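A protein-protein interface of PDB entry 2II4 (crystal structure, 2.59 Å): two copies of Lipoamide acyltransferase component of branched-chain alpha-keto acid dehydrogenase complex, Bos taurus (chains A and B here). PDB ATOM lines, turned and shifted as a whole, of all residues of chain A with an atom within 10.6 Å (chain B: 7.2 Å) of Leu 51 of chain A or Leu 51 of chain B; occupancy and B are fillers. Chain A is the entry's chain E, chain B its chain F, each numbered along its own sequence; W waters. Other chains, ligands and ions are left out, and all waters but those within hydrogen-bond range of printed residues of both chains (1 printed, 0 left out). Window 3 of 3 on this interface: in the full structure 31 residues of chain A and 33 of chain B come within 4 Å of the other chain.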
ATOM      1  N   MET A  43      14.959 -16.373  12.958  1.00  0.00           N
ATOM      2  CA  MET A  43      14.875 -17.733  12.481  1.00  0.00           C
ATOM      3  C   MET A  43      14.327 -17.808  11.031  1.00  0.00           C
ATOM      4  O   MET A  43      14.786 -18.646  10.256  1.00  0.00           O
ATOM      5  CB  MET A  43      14.089 -18.617  13.451  1.00  0.00           C
ATOM      6  CG  MET A  43      14.156 -20.050  13.113  1.00  0.00           C
ATOM      7  SD  MET A  43      13.498 -21.149  14.391  1.00  0.00           S
ATOM      8  CE  MET A  43      11.700 -21.101  14.222  1.00  0.00           C
ATOM      9  N   VAL A  44      13.382 -16.942  10.664  1.00  0.00           N
ATOM     10  CA  VAL A  44      12.833 -16.980   9.316  1.00  0.00           C
ATOM     11  C   VAL A  44      13.992 -16.664   8.345  1.00  0.00           C
ATOM     12  O   VAL A  44      14.206 -17.347   7.324  1.00  0.00           O
ATOM     13  CB  VAL A  44      11.625 -15.978   9.092  1.00  0.00           C
ATOM     14  CG1 VAL A  44      11.107 -16.056   7.646  1.00  0.00           C
ATOM     15  CG2 VAL A  44      10.439 -16.239  10.048  1.00  0.00           C
ATOM     16  N   LYS A  45      14.762 -15.643   8.700  1.00  0.00           N
ATOM     17  CA  LYS A  45      15.852 -15.185   7.842  1.00  0.00           C
ATOM     18  C   LYS A  45      16.918 -16.247   7.776  1.00  0.00           C
ATOM     19  O   LYS A  45      17.341 -16.651   6.681  1.00  0.00           O
ATOM     20  CB  LYS A  45      16.407 -13.813   8.275  1.00  0.00           C
ATOM     21  CG  LYS A  45      15.793 -12.682   7.444  1.00  0.00           C
ATOM     22  CD  LYS A  45      15.752 -11.275   8.132  1.00  0.00           C
ATOM     23  CE  LYS A  45      14.817 -10.291   7.297  1.00  0.00           C
ATOM     24  NZ  LYS A  45      15.231  -8.817   7.305  1.00  0.00           N
ATOM     25  N   THR A  46      17.259 -16.771   8.938  1.00  0.00           N
ATOM     26  CA  THR A  46      18.311 -17.765   9.055  1.00  0.00           C
ATOM     27  C   THR A  46      18.012 -19.078   8.317  1.00  0.00           C
ATOM     28  O   THR A  46      18.764 -19.522   7.439  1.00  0.00           O
ATOM     29  CB  THR A  46      18.680 -17.931  10.533  1.00  0.00           C
ATOM     30  OG1 THR A  46      19.683 -16.971  10.854  1.00  0.00           O
ATOM     31  CG2 THR A  46      19.265 -19.190  10.788  1.00  0.00           C
ATOM     32  N   MET A  47      16.904 -19.700   8.662  1.00  0.00           N
ATOM     33  CA  MET A  47      16.541 -20.915   7.995  1.00  0.00           C
ATOM     34  C   MET A  47      16.334 -20.664   6.503  1.00  0.00           C
ATOM     35  O   MET A  47      16.585 -21.529   5.696  1.00  0.00           O
ATOM     36  CB  MET A  47      15.298 -21.522   8.612  1.00  0.00           C
ATOM     37  CG  MET A  47      15.491 -22.011  10.003  1.00  0.00           C
ATOM     38  SD  MET A  47      17.045 -22.820  10.253  1.00  0.00           S
ATOM     39  CE  MET A  47      17.158 -22.730  12.017  1.00  0.00           C
ATOM     40  N   SER A  48      15.873 -19.494   6.118  1.00  0.00           N
ATOM     41  CA  SER A  48      15.751 -19.283   4.682  1.00  0.00           C
ATOM     42  C   SER A  48      17.080 -19.348   3.924  1.00  0.00           C
ATOM     43  O   SER A  48      17.145 -19.917   2.832  1.00  0.00           O
ATOM     44  CB  SER A  48      15.045 -17.973   4.380  1.00  0.00           C
ATOM     45  OG  SER A  48      13.699 -18.133   4.737  1.00  0.00           O
ATOM     46  N   ALA A  49      18.123 -18.772   4.507  1.00  0.00           N
ATOM     47  CA  ALA A  49      19.388 -18.709   3.845  1.00  0.00           C
ATOM     48  C   ALA A  49      19.959 -20.143   3.800  1.00  0.00           C
ATOM     49  O   ALA A  49      20.632 -20.542   2.817  1.00  0.00           O
ATOM     50  CB  ALA A  49      20.294 -17.748   4.546  1.00  0.00           C
ATOM     51  N   ALA A  50      19.624 -20.937   4.820  1.00  0.00           N
ATOM     52  CA  ALA A  50      20.051 -22.333   4.853  1.00  0.00           C
ATOM     53  C   ALA A  50      19.541 -23.131   3.669  1.00  0.00           C
ATOM     54  O   ALA A  50      20.059 -24.199   3.358  1.00  0.00           O
ATOM     55  CB  ALA A  50      19.612 -22.984   6.147  1.00  0.00           C
ATOM     56  N   LEU A  51      18.533 -22.612   2.984  1.00  0.00           N
ATOM     57  CA  LEU A  51      18.055 -23.286   1.778  1.00  0.00           C
ATOM     58  C   LEU A  51      19.107 -23.270   0.682  1.00  0.00           C
ATOM     59  O   LEU A  51      18.969 -23.975  -0.296  1.00  0.00           O
ATOM     60  CB  LEU A  51      16.786 -22.655   1.237  1.00  0.00           C
ATOM     61  CG  LEU A  51      15.483 -22.899   1.974  1.00  0.00           C
ATOM     62  CD1 LEU A  51      14.409 -21.965   1.330  1.00  0.00           C
ATOM     63  CD2 LEU A  51      15.041 -24.384   1.974  1.00  0.00           C
ATOM     64  N   LYS A  52      20.134 -22.438   0.815  1.00  0.00           N
ATOM     65  CA  LYS A  52      21.162 -22.403  -0.219  1.00  0.00           C
ATOM     66  C   LYS A  52      22.243 -23.483  -0.034  1.00  0.00           C
ATOM     67  O   LYS A  52      23.081 -23.674  -0.908  1.00  0.00           O
ATOM     68  CB  LYS A  52      21.769 -21.015  -0.352  1.00  0.00           C
ATOM     69  CG  LYS A  52      20.879 -19.977  -1.024  1.00  0.00           C
ATOM     70  CD  LYS A  52      21.418 -18.572  -0.656  1.00  0.00           C
ATOM     71  CE  LYS A  52      20.559 -17.347  -1.174  1.00  0.00           C
ATOM     72  NZ  LYS A  52      20.003 -17.523  -2.576  1.00  0.00           N
ATOM     73  N   ILE A  53      22.194 -24.201   1.090  1.00  0.00           N
ATOM     74  CA  ILE A  53      23.173 -25.211   1.400  1.00  0.00           C
ATOM     75  C   ILE A  53      22.576 -26.558   1.111  1.00  0.00           C
ATOM     76  O   ILE A  53      21.582 -26.901   1.741  1.00  0.00           O
ATOM     77  CB  ILE A  53      23.494 -25.226   2.892  1.00  0.00           C
ATOM     78  CG1 ILE A  53      24.042 -23.870   3.344  1.00  0.00           C
ATOM     79  CG2 ILE A  53      24.504 -26.351   3.221  1.00  0.00           C
ATOM     80  CD1 ILE A  53      24.288 -23.762   4.907  1.00  0.00           C
ATOM     81  N   PRO A  54      23.197 -27.353   0.208  1.00  0.00           N
ATOM     82  CA  PRO A  54      22.834 -28.767  -0.003  1.00  0.00           C
ATOM     83  C   PRO A  54      23.270 -29.567   1.193  1.00  0.00           C
ATOM     84  O   PRO A  54      24.458 -29.735   1.401  1.00  0.00           O
ATOM     85  CB  PRO A  54      23.670 -29.198  -1.206  1.00  0.00           C
ATOM     86  CG  PRO A  54      24.236 -27.996  -1.757  1.00  0.00           C
ATOM     87  CD  PRO A  54      24.323 -26.967  -0.656  1.00  0.00           C
ATOM     88  N   HIS A  55      22.309 -30.011   1.993  1.00  0.00           N
ATOM     89  CA  HIS A  55      22.609 -30.710   3.248  1.00  0.00           C
ATOM     90  C   HIS A  55      22.901 -32.154   2.953  1.00  0.00           C
ATOM     91  O   HIS A  55      22.122 -32.801   2.285  1.00  0.00           O
ATOM     92  CB  HIS A  55      21.442 -30.601   4.222  1.00  0.00           C
ATOM     93  CG  HIS A  55      21.359 -29.271   4.915  1.00  0.00           C
ATOM     94  ND1 HIS A  55      21.240 -28.077   4.236  1.00  0.00           N
ATOM     95  CD2 HIS A  55      21.340 -28.953   6.234  1.00  0.00           C
ATOM     96  CE1 HIS A  55      21.176 -27.084   5.113  1.00  0.00           C
ATOM     97  NE2 HIS A  55      21.237 -27.588   6.330  1.00  0.00           N
ATOM     98  N   GLU A 111      29.342 -16.478  -0.772  1.00  0.00           N
ATOM     99  CA  GLU A 111      28.052 -16.617  -1.445  1.00  0.00           C
ATOM    100  C   GLU A 111      28.103 -17.647  -2.582  1.00  0.00           C
ATOM    101  O   GLU A 111      27.257 -18.558  -2.612  1.00  0.00           O
ATOM    102  CB  GLU A 111      27.550 -15.273  -1.970  1.00  0.00           C
ATOM    103  CG  GLU A 111      26.158 -15.373  -2.654  1.00  0.00           C
ATOM    104  CD  GLU A 111      25.013 -15.040  -1.685  1.00  0.00           C
ATOM    105  OE1 GLU A 111      24.938 -13.853  -1.264  1.00  0.00           O
ATOM    106  OE2 GLU A 111      24.202 -15.953  -1.349  1.00  0.00           O
ATOM    107  N   LYS A 190      17.230 -34.362  11.620  1.00  0.00           N
ATOM    108  CA  LYS A 190      17.835 -33.681  10.454  1.00  0.00           C
ATOM    109  C   LYS A 190      17.917 -32.219  10.788  1.00  0.00           C
ATOM    110  O   LYS A 190      16.998 -31.450  10.493  1.00  0.00           O
ATOM    111  CB  LYS A 190      17.089 -33.938   9.127  1.00  0.00           C
ATOM    112  CG  LYS A 190      17.766 -33.263   7.854  1.00  0.00           C
ATOM    113  CD  LYS A 190      17.080 -31.878   7.311  1.00  0.00           C
ATOM    114  CE  LYS A 190      17.867 -31.339   6.094  1.00  0.00           C
ATOM    115  NZ  LYS A 190      17.161 -30.361   5.098  1.00  0.00           N
ATOM    116  N   PRO A 191      19.006 -31.838  11.456  1.00  0.00           N
ATOM    117  CA  PRO A 191      19.307 -30.480  11.870  1.00  0.00           C
ATOM    118  C   PRO A 191      19.650 -29.630  10.662  1.00  0.00           C
ATOM    119  O   PRO A 191      20.212 -30.150   9.713  1.00  0.00           O
ATOM    120  CB  PRO A 191      20.558 -30.669  12.701  1.00  0.00           C
ATOM    121  CG  PRO A 191      21.218 -31.834  12.054  1.00  0.00           C
ATOM    122  CD  PRO A 191      20.076 -32.767  11.859  1.00  0.00           C
ATOM    123  N   VAL A 192      19.347 -28.332  10.718  1.00  0.00           N
ATOM    124  CA  VAL A 192      19.551 -27.407   9.595  1.00  0.00           C
ATOM    125  C   VAL A 192      20.764 -26.538   9.907  1.00  0.00           C
ATOM    126  O   VAL A 192      20.878 -26.007  11.011  1.00  0.00           O
ATOM    127  CB  VAL A 192      18.319 -26.524   9.406  1.00  0.00           C
ATOM    128  CG1 VAL A 192      18.544 -25.470   8.357  1.00  0.00           C
ATOM    129  CG2 VAL A 192      17.123 -27.373   9.041  1.00  0.00           C
ATOM    130  N   ILE A 193      21.693 -26.427   8.969  1.00  0.00           N
ATOM    131  CA  ILE A 193      22.909 -25.704   9.215  1.00  0.00           C
ATOM    132  C   ILE A 193      22.625 -24.206   9.334  1.00  0.00           C
ATOM    133  O   ILE A 193      21.764 -23.673   8.646  1.00  0.00           O
ATOM    134  CB  ILE A 193      23.940 -25.950   8.069  1.00  0.00           C
ATOM    135  CG1 ILE A 193      24.169 -27.446   7.857  1.00  0.00           C
ATOM    136  CG2 ILE A 193      25.282 -25.246   8.358  1.00  0.00           C
ATOM    137  CD1 ILE A 193      24.945 -27.785   6.616  1.00  0.00           C
ATOM    138  N   LEU A 194      23.420 -23.529  10.153  1.00  0.00           N
ATOM    139  CA  LEU A 194      23.262 -22.124  10.415  1.00  0.00           C
ATOM    140  C   LEU A 194      24.297 -21.342   9.693  1.00  0.00           C
ATOM    141  O   LEU A 194      25.433 -21.267  10.154  1.00  0.00           O
ATOM    142  CB  LEU A 194      23.558 -21.905  11.871  1.00  0.00           C
ATOM    143  CG  LEU A 194      22.386 -21.743  12.793  1.00  0.00           C
ATOM    144  CD1 LEU A 194      21.261 -22.742  12.415  1.00  0.00           C
ATOM    145  CD2 LEU A 194      22.933 -21.989  14.216  1.00  0.00           C
ATOM    146  N   PRO A 195      23.925 -20.700   8.598  1.00  0.00           N
ATOM    147  CA  PRO A 195      24.910 -19.944   7.811  1.00  0.00           C
ATOM    148  C   PRO A 195      25.538 -18.844   8.691  1.00  0.00           C
ATOM    149  O   PRO A 195      24.814 -18.231   9.479  1.00  0.00           O
ATOM    150  CB  PRO A 195      24.066 -19.316   6.688  1.00  0.00           C
ATOM    151  CG  PRO A 195      22.803 -20.126   6.612  1.00  0.00           C
ATOM    152  CD  PRO A 195      22.565 -20.610   8.053  1.00  0.00           C
ATOM    153  N   GLU A 197      28.099 -21.090   8.929  1.00  0.00           N
ATOM    154  CA  GLU A 197      28.740 -22.360   9.273  1.00  0.00           C
ATOM    155  C   GLU A 197      28.479 -23.387   8.181  1.00  0.00           C
ATOM    156  O   GLU A 197      27.633 -23.172   7.279  1.00  0.00           O
ATOM    157  CB  GLU A 197      28.270 -22.854  10.626  1.00  0.00           C
ATOM    158  CG  GLU A 197      28.493 -21.806  11.682  1.00  0.00           C
ATOM    159  CD  GLU A 197      27.723 -22.021  12.965  1.00  0.00           C
ATOM    160  OE1 GLU A 197      27.156 -23.118  13.165  1.00  0.00           O
ATOM    161  OE2 GLU A 197      27.702 -21.059  13.797  1.00  0.00           O
ATOM    162  N   ASP A 231      27.489 -29.033   4.755  1.00  0.00           N
ATOM    163  CA  ASP A 231      27.422 -28.448   3.417  1.00  0.00           C
ATOM    164  C   ASP A 231      28.170 -29.303   2.400  1.00  0.00           C
ATOM    165  O   ASP A 231      29.387 -29.213   2.255  1.00  0.00           O
ATOM    166  CB  ASP A 231      28.023 -27.034   3.451  1.00  0.00           C
ATOM    167  CG  ASP A 231      27.801 -26.249   2.158  1.00  0.00           C
ATOM    168  OD1 ASP A 231      27.608 -26.820   1.058  1.00  0.00           O
ATOM    169  OD2 ASP A 231      27.834 -25.013   2.240  1.00  0.00           O
ATOM    170  N   ARG A 233      28.661 -29.107  -0.530  1.00  0.00           N
ATOM    171  CA  ARG A 233      29.355 -28.480  -1.635  1.00  0.00           C
ATOM    172  C   ARG A 233      30.864 -28.581  -1.475  1.00  0.00           C
ATOM    173  O   ARG A 233      31.578 -28.615  -2.475  1.00  0.00           O
ATOM    174  CB  ARG A 233      28.976 -27.009  -1.762  1.00  0.00           C
ATOM    175  CG  ARG A 233      27.614 -26.782  -2.349  1.00  0.00           C
ATOM    176  CD  ARG A 233      27.256 -25.357  -2.322  1.00  0.00           C
ATOM    177  NE  ARG A 233      27.278 -24.827  -0.957  1.00  0.00           N
ATOM    178  CZ  ARG A 233      26.948 -23.562  -0.675  1.00  0.00           C
ATOM    179  NH1 ARG A 233      26.601 -22.766  -1.675  1.00  0.00           N
ATOM    180  NH2 ARG A 233      26.971 -23.090   0.586  1.00  0.00           N
ATOM    181  N   THR B  46       3.387 -29.846  -6.391  1.00  0.00           N
ATOM    182  CA  THR B  46       3.392 -29.820  -4.934  1.00  0.00           C
ATOM    183  C   THR B  46       4.829 -29.970  -4.370  1.00  0.00           C
ATOM    184  O   THR B  46       5.282 -29.190  -3.539  1.00  0.00           O
ATOM    185  CB  THR B  46       2.447 -30.905  -4.443  1.00  0.00           C
ATOM    186  OG1 THR B  46       1.105 -30.503  -4.744  1.00  0.00           O
ATOM    187  CG2 THR B  46       2.551 -31.076  -2.994  1.00  0.00           C
ATOM    188  N   MET B  47       5.563 -30.938  -4.880  1.00  0.00           N
ATOM    189  CA  MET B  47       6.938 -31.180  -4.426  1.00  0.00           C
ATOM    190  C   MET B  47       7.883 -30.055  -4.798  1.00  0.00           C
ATOM    191  O   MET B  47       8.804 -29.791  -4.066  1.00  0.00           O
ATOM    192  CB  MET B  47       7.486 -32.540  -4.904  1.00  0.00           C
ATOM    193  CG  MET B  47       6.749 -33.723  -4.317  1.00  0.00           C
ATOM    194  SD  MET B  47       6.455 -33.599  -2.535  1.00  0.00           S
ATOM    195  CE  MET B  47       4.865 -34.402  -2.491  1.00  0.00           C
ATOM    196  N   SER B  48       7.644 -29.374  -5.904  1.00  0.00           N
ATOM    197  CA  SER B  48       8.512 -28.266  -6.282  1.00  0.00           C
ATOM    198  C   SER B  48       8.291 -27.111  -5.341  1.00  0.00           C
ATOM    199  O   SER B  48       9.229 -26.439  -4.959  1.00  0.00           O
ATOM    200  CB  SER B  48       8.306 -27.810  -7.747  1.00  0.00           C
ATOM    201  OG  SER B  48       8.760 -28.817  -8.683  1.00  0.00           O
ATOM    202  N   ALA B  49       7.044 -26.880  -4.948  1.00  0.00           N
ATOM    203  CA  ALA B  49       6.740 -25.761  -4.073  1.00  0.00           C
ATOM    204  C   ALA B  49       7.372 -26.075  -2.665  1.00  0.00           C
ATOM    205  O   ALA B  49       7.826 -25.176  -1.953  1.00  0.00           O
ATOM    206  CB  ALA B  49       5.221 -25.578  -4.008  1.00  0.00           C
ATOM    207  N   ALA B  50       7.410 -27.361  -2.296  1.00  0.00           N
ATOM    208  CA  ALA B  50       8.049 -27.793  -1.045  1.00  0.00           C
ATOM    209  C   ALA B  50       9.532 -27.385  -0.891  1.00  0.00           C
ATOM    210  O   ALA B  50      10.017 -27.169   0.233  1.00  0.00           O
ATOM    211  CB  ALA B  50       7.860 -29.290  -0.838  1.00  0.00           C
ATOM    212  N   LEU B  51      10.244 -27.233  -2.003  1.00  0.00           N
ATOM    213  CA  LEU B  51      11.618 -26.722  -1.932  1.00  0.00           C
ATOM    214  C   LEU B  51      11.762 -25.403  -1.204  1.00  0.00           C
ATOM    215  O   LEU B  51      12.829 -25.062  -0.698  1.00  0.00           O
ATOM    216  CB  LEU B  51      12.202 -26.544  -3.334  1.00  0.00           C
ATOM    217  CG  LEU B  51      12.486 -27.849  -4.073  1.00  0.00           C
ATOM    218  CD1 LEU B  51      12.645 -27.589  -5.598  1.00  0.00           C
ATOM    219  CD2 LEU B  51      13.692 -28.546  -3.403  1.00  0.00           C
ATOM    220  N   LYS B  52      10.703 -24.617  -1.206  1.00  0.00           N
ATOM    221  CA  LYS B  52      10.732 -23.341  -0.520  1.00  0.00           C
ATOM    222  C   LYS B  52      10.680 -23.486   1.022  1.00  0.00           C
ATOM    223  O   LYS B  52      10.961 -22.526   1.759  1.00  0.00           O
ATOM    224  CB  LYS B  52       9.588 -22.484  -1.025  1.00  0.00           C
ATOM    225  CG  LYS B  52       9.770 -21.949  -2.440  1.00  0.00           C
ATOM    226  CD  LYS B  52       8.517 -21.113  -2.742  1.00  0.00           C
ATOM    227  CE  LYS B  52       8.665 -20.324  -4.045  1.00  0.00           C
ATOM    228  NZ  LYS B  52       7.951 -21.074  -5.123  1.00  0.00           N
ATOM    229  N   ILE B  53      10.351 -24.675   1.508  1.00  0.00           N
ATOM    230  CA  ILE B  53      10.300 -24.870   2.931  1.00  0.00           C
ATOM    231  C   ILE B  53      11.588 -25.447   3.451  1.00  0.00           C
ATOM    232  O   ILE B  53      12.061 -26.466   2.968  1.00  0.00           O
ATOM    233  CB  ILE B  53       9.192 -25.813   3.302  1.00  0.00           C
ATOM    234  CG1 ILE B  53       7.858 -25.345   2.757  1.00  0.00           C
ATOM    235  CG2 ILE B  53       9.094 -25.918   4.757  1.00  0.00           C
ATOM    236  CD1 ILE B  53       6.824 -26.383   2.969  1.00  0.00           C
ATOM    237  N   PRO B  54      12.223 -24.775   4.393  1.00  0.00           N
ATOM    238  CA  PRO B  54      13.402 -25.413   5.037  1.00  0.00           C
ATOM    239  C   PRO B  54      12.965 -26.445   6.050  1.00  0.00           C
ATOM    240  O   PRO B  54      12.394 -26.069   7.093  1.00  0.00           O
ATOM    241  CB  PRO B  54      14.127 -24.260   5.748  1.00  0.00           C
ATOM    242  CG  PRO B  54      13.278 -23.111   5.640  1.00  0.00           C
ATOM    243  CD  PRO B  54      11.989 -23.410   4.860  1.00  0.00           C
ATOM    244  N   HIS B  55      13.219 -27.715   5.731  1.00  0.00           N
ATOM    245  CA  HIS B  55      12.743 -28.836   6.510  1.00  0.00           C
ATOM    246  C   HIS B  55      13.686 -29.180   7.661  1.00  0.00           C
ATOM    247  O   HIS B  55      14.882 -29.427   7.445  1.00  0.00           O
ATOM    248  CB  HIS B  55      12.628 -30.080   5.651  1.00  0.00           C
ATOM    249  CG  HIS B  55      11.463 -30.083   4.733  1.00  0.00           C
ATOM    250  ND1 HIS B  55      11.323 -29.172   3.707  1.00  0.00           N
ATOM    251  CD2 HIS B  55      10.403 -30.921   4.648  1.00  0.00           C
ATOM    252  CE1 HIS B  55      10.202 -29.424   3.050  1.00  0.00           C
ATOM    253  NE2 HIS B  55       9.627 -30.486   3.597  1.00  0.00           N
ATOM    254  N   VAL B 192       8.216 -35.102   3.081  1.00  0.00           N
ATOM    255  CA  VAL B 192       8.196 -33.770   2.499  1.00  0.00           C
ATOM    256  C   VAL B 192       6.850 -33.097   2.883  1.00  0.00           C
ATOM    257  O   VAL B 192       5.792 -33.624   2.589  1.00  0.00           O
ATOM    258  CB  VAL B 192       8.368 -33.870   0.961  1.00  0.00           C
ATOM    259  CG1 VAL B 192       8.015 -32.578   0.325  1.00  0.00           C
ATOM    260  CG2 VAL B 192       9.798 -34.231   0.572  1.00  0.00           C
ATOM    261  N   ILE B 193       6.925 -31.973   3.590  1.00  0.00           N
ATOM    262  CA  ILE B 193       5.768 -31.183   3.934  1.00  0.00           C
ATOM    263  C   ILE B 193       5.023 -30.831   2.637  1.00  0.00           C
ATOM    264  O   ILE B 193       5.653 -30.517   1.633  1.00  0.00           O
ATOM    265  CB  ILE B 193       6.207 -29.879   4.666  1.00  0.00           C
ATOM    266  CG1 ILE B 193       7.051 -30.194   5.918  1.00  0.00           C
ATOM    267  CG2 ILE B 193       5.004 -28.989   5.061  1.00  0.00           C
ATOM    268  CD1 ILE B 193       7.756 -28.941   6.549  1.00  0.00           C
ATOM    269  N   PRO B 195       2.846 -28.152   1.015  1.00  0.00           N
ATOM    270  CA  PRO B 195       2.379 -26.761   1.151  1.00  0.00           C
ATOM    271  C   PRO B 195       0.878 -26.724   0.919  1.00  0.00           C
ATOM    272  O   PRO B 195       0.393 -27.531   0.127  1.00  0.00           O
ATOM    273  CB  PRO B 195       3.058 -26.038  -0.004  1.00  0.00           C
ATOM    274  CG  PRO B 195       4.230 -26.840  -0.312  1.00  0.00           C
ATOM    275  CD  PRO B 195       3.874 -28.295  -0.016  1.00  0.00           C
ATOM    276  N   ARG B 233      11.220 -22.302   9.497  1.00  0.00           N
ATOM    277  CA  ARG B 233      11.115 -20.850   9.533  1.00  0.00           C
ATOM    278  C   ARG B 233      10.343 -20.381  10.786  1.00  0.00           C
ATOM    279  O   ARG B 233      10.714 -19.358  11.440  1.00  0.00           O
ATOM    280  CB  ARG B 233      10.462 -20.312   8.236  1.00  0.00           C
ATOM    281  CG  ARG B 233      11.405 -20.457   7.072  1.00  0.00           C
ATOM    282  CD  ARG B 233      10.765 -20.201   5.787  1.00  0.00           C
ATOM    283  NE  ARG B 233       9.571 -20.998   5.553  1.00  0.00           N
ATOM    284  CZ  ARG B 233       8.730 -20.710   4.553  1.00  0.00           C
ATOM    285  NH1 ARG B 233       9.014 -19.669   3.753  1.00  0.00           N
ATOM    286  NH2 ARG B 233       7.625 -21.438   4.341  1.00  0.00           N
HETATM  287  O   HOH W   1      11.181 -18.137   3.607  1.00  0.00           O
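Water W1 bridges NH1 of Arg 233 of chain B (2.7 Å) and OG of Ser 48 of chain A (2.8 Å).
Met 47 of chain A touches Pro 54 of chain B, but with the chains exchanged Pro 54 of chain A does not touch Met 47 of chain B (14.6 Å).
Leu 51 of chain A touches Lys 52 of chain B, but with the chains exchanged Lys 52 of chain A does not touch Leu 51 of chain B (7.9 Å).
Leu 51 of chain A touches Pro 54 of chain B, but with the chains exchanged Pro 54 of chain A does not touch Leu 51 of chain B (9.8 Å).
Val 192 of chain A touches His 55 of chain B, but with the chains exchanged His 55 of chain A does not touch Val 192 of chain B (12.5 Å).
14 positions are printed for both chains.
Of the 10 pairs that touch across the chains among the printed residues, 1 has its exchanged pair printed and touching as well.
The backbone carbonyl oxygen of Val 44 of chain A lies within hydrogen-bond range of the side-chain hydroxyl of Ser 48 of chain A (2.8 Å).
A ring nitrogen (ND1) of His 55 of chain B lies within hydrogen-bond range of the backbone carbonyl oxygen of Ile 53 of chain B, 2.9 Å away.
N of Ile 193 of chain B sits at hydrogen-bond distance from NE2 of His 55 of chain B.
O of His 55 of chain B lies close to NZ of Lys 190 of chain A (3.4 Å).
Among the printed residues, merely in contact across the chains: Val 44 of chain A with Arg 233 of chain B (3.4 Å), Met 43 of chain A with Arg 233 of chain B (3.4 Å), Val 192 of chain A with His 55 of chain B (3.4 Å), Leu 51 of chain A with Lys 52 of chain B (3.5 Å), Leu 51 of chain A with Leu 51 of chain B (3.5 Å), Leu 51 of chain A with Pro 54 of chain B (3.6 Å), Met 47 of chain A with Pro 54 of chain B (3.7 Å), Ser 48 of chain A with Arg 233 of chain B (3.7 Å) and Leu 51 of chain A with Ile 53 of chain B (3.8 Å).
Of the printed residues of chain B, Met 47 of chain A touches Pro 54 (3.7 Å).
Of chain B, only Leu 51 (3.5 Å), Lys 52 (3.5 Å), Ile 53 (3.8 Å) and Pro 54 (3.6 Å) come within 4 Å of Leu 51 of chain A.
No residue of chain A comes within 4 Å of Ala 50 of chain B.
Of the printed residues of chain A, Leu 51 of chain B touches Leu 51.
Of the printed residues of chain A, Lys 52 of chain B touches Leu 51.
Pro 54 of chain B touches two residues of chain A.
The nearest residue of chain B that does not touch Leu 51 of chain A is His 55 of chain B (5.3 Å).
The nearest printed residue of chain A that does not touch His 55 of chain B is Leu 51 of chain A (5.3 Å).
Printed residues of chain B that touch a printed residue of chain A: Leu 51, Lys 52, Ile 53, Pro 54, His 55 and Arg 233.
Hydrophobic or aromatic side chains of chain B that line the printed part of chain A: Pro 54.
Of the 23 printed residues of chain A, 7 touch a printed residue of chain B.
Along chain A the printed residues that touch a printed residue of chain B span positions 43 to 192.
Among the printed residues, no Asp or Glu carboxylate lies within 4 Å of a Lys or Arg side-chain nitrogen of the other chain.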
